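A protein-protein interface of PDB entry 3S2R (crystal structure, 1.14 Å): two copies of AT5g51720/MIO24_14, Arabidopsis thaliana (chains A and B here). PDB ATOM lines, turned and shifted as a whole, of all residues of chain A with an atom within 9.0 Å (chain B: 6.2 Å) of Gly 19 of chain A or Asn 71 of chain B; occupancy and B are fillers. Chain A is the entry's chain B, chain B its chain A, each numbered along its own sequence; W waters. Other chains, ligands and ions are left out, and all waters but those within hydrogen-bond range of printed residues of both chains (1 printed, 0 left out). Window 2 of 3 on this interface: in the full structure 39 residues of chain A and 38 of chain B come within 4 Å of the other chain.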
ATOM      1  N   ALA A  15      22.184  -7.431  10.693  1.00  0.00           N
ATOM      2  CA  ALA A  15      21.944  -8.101  11.957  1.00  0.00           C
ATOM      3  C   ALA A  15      21.236  -7.028  12.721  1.00  0.00           C
ATOM      4  O   ALA A  15      21.199  -5.882  12.273  1.00  0.00           O
ATOM      5  CB  ALA A  15      23.272  -8.489  12.598  1.00  0.00           C
ATOM      6  N   GLU A  16      20.628  -7.380  13.846  1.00  0.00           N
ATOM      7  CA  GLU A  16      20.034  -6.391  14.770  1.00  0.00           C
ATOM      8  C   GLU A  16      19.095  -5.282  14.267  1.00  0.00           C
ATOM      9  O   GLU A  16      18.100  -5.526  13.579  1.00  0.00           O
ATOM     10  CB  GLU A  16      21.123  -5.747  15.633  1.00  0.00           C
ATOM     11  CG  GLU A  16      21.050  -6.151  17.091  1.00  0.00           C
ATOM     12  CD  GLU A  16      21.062  -4.975  18.065  1.00  0.00           C
ATOM     13  OE1 GLU A  16      20.543  -5.148  19.179  1.00  0.00           O
ATOM     14  OE2 GLU A  16      21.588  -3.883  17.731  1.00  0.00           O
ATOM     15  N   GLY A  17      19.431  -4.063  14.639  1.00  0.00           N
ATOM     16  CA  GLY A  17      18.604  -2.913  14.429  1.00  0.00           C
ATOM     17  C   GLY A  17      19.373  -1.951  13.574  1.00  0.00           C
ATOM     18  O   GLY A  17      19.349  -2.047  12.350  1.00  0.00           O
ATOM     19  N   GLY A  18      20.084  -1.038  14.232  1.00  0.00           N
ATOM     20  CA  GLY A  18      20.519   0.191  13.586  1.00  0.00           C
ATOM     21  C   GLY A  18      19.343   1.145  13.722  1.00  0.00           C
ATOM     22  O   GLY A  18      18.330   0.802  14.346  1.00  0.00           O
ATOM     23  N   GLY A  19      19.463   2.335  13.147  1.00  0.00           N
ATOM     24  CA  GLY A  19      18.423   3.356  13.301  1.00  0.00           C
ATOM     25  C   GLY A  19      17.349   3.329  12.230  1.00  0.00           C
ATOM     26  O   GLY A  19      16.256   3.888  12.419  1.00  0.00           O
ATOM     27  N   GLY A  20      17.645   2.653  11.121  1.00  0.00           N
ATOM     28  CA  GLY A  20      16.796   2.661   9.925  1.00  0.00           C
ATOM     29  C   GLY A  20      15.494   1.899  10.052  1.00  0.00           C
ATOM     30  O   GLY A  20      15.325   1.047  10.944  1.00  0.00           O
ATOM     31  N   ILE A  21      14.582   2.180   9.132  1.00  0.00           N
ATOM     32  CA  ILE A  21      13.315   1.444   9.086  1.00  0.00           C
ATOM     33  C   ILE A  21      13.054   0.753   7.744  1.00  0.00           C
ATOM     34  O   ILE A  21      12.082  -0.019   7.639  1.00  0.00           O
ATOM     35  CB  ILE A  21      12.117   2.318   9.400  1.00  0.00           C
ATOM     36  CG1 ILE A  21      11.932   3.412   8.349  1.00  0.00           C
ATOM     37  CG2 ILE A  21      12.222   2.909  10.784  1.00  0.00           C
ATOM     38  CD1 ILE A  21      10.574   4.201   8.448  1.00  0.00           C
ATOM     39  N   ASN A  22      13.868   1.039   6.726  1.00  0.00           N
ATOM     40  CA  ASN A  22      13.741   0.455   5.404  1.00  0.00           C
ATOM     41  C   ASN A  22      15.040  -0.284   5.043  1.00  0.00           C
ATOM     42  O   ASN A  22      15.866   0.258   4.333  1.00  0.00           O
ATOM     43  CB  ASN A  22      13.418   1.515   4.343  1.00  0.00           C
ATOM     44  CG  ASN A  22      13.432   0.962   2.964  1.00  0.00           C
ATOM     45  OD1 ASN A  22      13.050  -0.190   2.746  1.00  0.00           O
ATOM     46  ND2 ASN A  22      13.826   1.783   2.002  1.00  0.00           N
ATOM     47  N   PRO A  23      15.185  -1.546   5.454  1.00  0.00           N
ATOM     48  CA  PRO A  23      16.438  -2.225   5.119  1.00  0.00           C
ATOM     49  C   PRO A  23      16.600  -2.615   3.653  1.00  0.00           C
ATOM     50  O   PRO A  23      17.728  -2.801   3.230  1.00  0.00           O
ATOM     51  CB  PRO A  23      16.413  -3.489   6.000  1.00  0.00           C
ATOM     52  CG  PRO A  23      14.958  -3.685   6.387  1.00  0.00           C
ATOM     53  CD  PRO A  23      14.347  -2.305   6.412  1.00  0.00           C
ATOM     54  N   LYS A  27      16.983   0.838  -2.277  1.00  0.00           N
ATOM     55  CA  LYS A  27      18.079   1.430  -1.521  1.00  0.00           C
ATOM     56  C   LYS A  27      19.021   2.276  -2.387  1.00  0.00           C
ATOM     57  O   LYS A  27      19.848   3.046  -1.876  1.00  0.00           O
ATOM     58  CB  LYS A  27      18.816   0.358  -0.695  1.00  0.00           C
ATOM     59  CG  LYS A  27      17.890  -0.416   0.307  1.00  0.00           C
ATOM     60  CD  LYS A  27      17.151   0.530   1.266  1.00  0.00           C
ATOM     61  CE  LYS A  27      18.118   1.214   2.209  1.00  0.00           C
ATOM     62  NZ  LYS A  27      17.464   2.121   3.183  1.00  0.00           N
ATOM     63  N   ARG B  53       7.764   9.450  12.170  1.00  0.00           N
ATOM     64  CA  ARG B  53       8.500  10.437  12.977  1.00  0.00           C
ATOM     65  C   ARG B  53       7.860  11.824  12.926  1.00  0.00           C
ATOM     66  O   ARG B  53       8.290  12.703  13.662  1.00  0.00           O
ATOM     67  CB  ARG B  53       9.986  10.561  12.554  1.00  0.00           C
ATOM     68  CG  ARG B  53      10.838   9.292  12.433  1.00  0.00           C
ATOM     69  CD  ARG B  53      10.710   8.544  13.684  1.00  0.00           C
ATOM     70  NE  ARG B  53      11.737   7.510  13.946  1.00  0.00           N
ATOM     71  CZ  ARG B  53      11.668   6.227  13.565  1.00  0.00           C
ATOM     72  NH1 ARG B  53      10.669   5.784  12.799  1.00  0.00           N
ATOM     73  NH2 ARG B  53      12.586   5.365  13.988  1.00  0.00           N
ATOM     74  N   LYS B  66      15.541  14.401   8.533  1.00  0.00           N
ATOM     75  CA  LYS B  66      16.437  14.377   9.677  1.00  0.00           C
ATOM     76  C   LYS B  66      16.728  12.941  10.056  1.00  0.00           C
ATOM     77  O   LYS B  66      17.858  12.605  10.375  1.00  0.00           O
ATOM     78  CB  LYS B  66      15.825  15.141  10.825  1.00  0.00           C
ATOM     79  CG  LYS B  66      15.571  16.591  10.461  1.00  0.00           C
ATOM     80  CD  LYS B  66      14.551  17.152  11.389  1.00  0.00           C
ATOM     81  CE  LYS B  66      14.324  18.619  11.142  1.00  0.00           C
ATOM     82  NZ  LYS B  66      13.700  19.189  12.363  1.00  0.00           N
ATOM     83  N   HIS B  67      15.695  12.097  10.039  1.00  0.00           N
ATOM     84  CA  HIS B  67      15.861  10.675  10.299  1.00  0.00           C
ATOM     85  C   HIS B  67      16.852  10.010   9.340  1.00  0.00           C
ATOM     86  O   HIS B  67      17.744   9.251   9.775  1.00  0.00           O
ATOM     87  CB  HIS B  67      14.500   9.978  10.261  1.00  0.00           C
ATOM     88  CG  HIS B  67      14.600   8.497  10.099  1.00  0.00           C
ATOM     89  ND1 HIS B  67      14.807   7.646  11.158  1.00  0.00           N
ATOM     90  CD2 HIS B  67      14.586   7.719   8.988  1.00  0.00           C
ATOM     91  CE1 HIS B  67      14.901   6.404  10.721  1.00  0.00           C
ATOM     92  NE2 HIS B  67      14.793   6.419   9.404  1.00  0.00           N
ATOM     93  N   ASN B  68      16.708  10.306   8.044  1.00  0.00           N
ATOM     94  CA  ASN B  68      17.538   9.743   6.989  1.00  0.00           C
ATOM     95  C   ASN B  68      19.016  10.124   7.205  1.00  0.00           C
ATOM     96  O   ASN B  68      19.937   9.281   7.100  1.00  0.00           O
ATOM     97  CB  ASN B  68      17.078  10.171   5.609  1.00  0.00           C
ATOM     98  CG  ASN B  68      15.848   9.458   5.162  1.00  0.00           C
ATOM     99  OD1 ASN B  68      15.487   8.401   5.687  1.00  0.00           O
ATOM    100  ND2 ASN B  68      15.182  10.019   4.158  1.00  0.00           N
ATOM    101  N   LYS B  69      19.229  11.398   7.542  1.00  0.00           N
ATOM    102  CA  LYS B  69      20.578  11.917   7.804  1.00  0.00           C
ATOM    103  C   LYS B  69      21.212  11.236   9.013  1.00  0.00           C
ATOM    104  O   LYS B  69      22.367  10.753   8.923  1.00  0.00           O
ATOM    105  CB  LYS B  69      20.536  13.427   8.038  1.00  0.00           C
ATOM    106  CG  LYS B  69      21.831  14.025   8.549  1.00  0.00           C
ATOM    107  CD  LYS B  69      22.567  14.783   7.453  1.00  0.00           C
ATOM    108  CE  LYS B  69      23.943  15.274   7.918  1.00  0.00           C
ATOM    109  NZ  LYS B  69      24.962  14.178   7.993  1.00  0.00           N
ATOM    110  N   ALA B  70      20.459  11.199  10.124  1.00  0.00           N
ATOM    111  CA  ALA B  70      20.937  10.609  11.378  1.00  0.00           C
ATOM    112  C   ALA B  70      21.205   9.117  11.281  1.00  0.00           C
ATOM    113  O   ALA B  70      22.217   8.652  11.827  1.00  0.00           O
ATOM    114  CB  ALA B  70      19.999  10.923  12.527  1.00  0.00           C
ATOM    115  N   ASN B  71      20.369   8.379  10.551  1.00  0.00           N
ATOM    116  CA  ASN B  71      20.381   6.915  10.579  1.00  0.00           C
ATOM    117  C   ASN B  71      20.812   6.256   9.259  1.00  0.00           C
ATOM    118  O   ASN B  71      20.724   5.038   9.113  1.00  0.00           O
ATOM    119  CB  ASN B  71      19.004   6.411  11.035  1.00  0.00           C
ATOM    120  CG  ASN B  71      18.679   6.836  12.456  1.00  0.00           C
ATOM    121  OD1 ASN B  71      19.260   6.320  13.406  1.00  0.00           O
ATOM    122  ND2 ASN B  71      17.764   7.787  12.604  1.00  0.00           N
ATOM    123  N   GLY B  72      21.311   7.051   8.318  1.00  0.00           N
ATOM    124  CA  GLY B  72      21.674   6.562   6.987  1.00  0.00           C
ATOM    125  C   GLY B  72      20.523   5.832   6.286  1.00  0.00           C
ATOM    126  O   GLY B  72      20.732   4.798   5.655  1.00  0.00           O
ATOM    127  N   ASP B  73      19.314   6.388   6.356  1.00  0.00           N
ATOM    128  CA  ASP B  73      18.144   5.763   5.764  1.00  0.00           C
ATOM    129  C   ASP B  73      17.710   6.550   4.506  1.00  0.00           C
ATOM    130  O   ASP B  73      18.309   7.566   4.169  1.00  0.00           O
ATOM    131  CB  ASP B  73      17.049   5.701   6.847  1.00  0.00           C
ATOM    132  CG  ASP B  73      16.059   4.550   6.645  1.00  0.00           C
ATOM    133  OD1 ASP B  73      16.175   3.793   5.637  1.00  0.00           O
ATOM    134  OD2 ASP B  73      15.194   4.357   7.534  1.00  0.00           O
HETATM  135  O   HOH W   1      17.299   1.436   6.791  1.00  0.00           O
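No position is printed for both chains. Of the 8 pairs that touch across the chains among the printed residues, none has its exchanged pair printed and touching as well.
Of the 9 printed residues of chain B, 4 touch a printed residue of chain A. Along chain B the printed residues that touch a printed residue of chain A span positions 53 to 73. Of the 10 printed residues of chain A, 5 touch a printed residue of chain B.
Of chain B, only His 67 (3.3 Å) and Asn 71 (3.1 Å) come within 4 Å of Gly 19 of chain A. Printed residues of chain A within 4 Å of Asn 71 of chain B: Gly 19 and Gly 20. No residue of chain A comes within 4 Å of Ala 70 of chain B. No residue of chain A comes within 4 Å of Gly 72 of chain B. Printed residues of chain B within 4 Å of Gly 20 of chain A: Asn 71 (3.997 Å) and Asp 73 (3.3 Å). Of the printed residues of chain B, Lys 27 of chain A touches Asp 73 (3.2 Å).
The side-chain carboxylate of Asp 73 of chain B sits at hydrogen-bond distance from the backbone NH of Ile 21 of chain A (2.8 Å). The side-chain carboxylate (OD1) of Asp 73 of chain B lies within salt-bridge range of the side-chain amino group (NZ) of Lys 27 of chain A (3.2 Å).
ND2 of Asn 71 of chain B sits at hydrogen-bond distance from O of His 67 of chain B (3.2 Å). A ring nitrogen (NE2) of His 67 of chain B is in hydrogen-bond range of the side-chain carboxylate (OD2) of Asp 73 of chain B (2.8 Å). O of Asn 68 of chain B lies within hydrogen-bond range of N of Asp 73 of chain B (3.1 Å). The backbone carbonyl oxygen (O) of Asn 22 of chain A is in hydrogen-bond range of the side-chain amino group (NZ) of Lys 27 of chain A (2.7 Å).
Water W1 lies within hydrogen-bond range of OD1 of Asp 73 of chain B (2.9 Å) and O of Asn 22 of chain A (3.1 Å).
Among the printed residues, pairs that only touch across the chains: Gly 19 of chain A with Asn 71 of chain B (3.1 Å), Gly 19 of chain A with His 67 of chain B (3.3 Å), Gly 20 of chain A with Asp 73 of chain B (3.3 Å), Asn 22 of chain A with Asp 73 of chain B (3.7 Å), Ile 21 of chain A with Arg 53 of chain B (3.8 Å) and Gly 20 of chain A with Asn 71 of chain B (3.997 Å).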
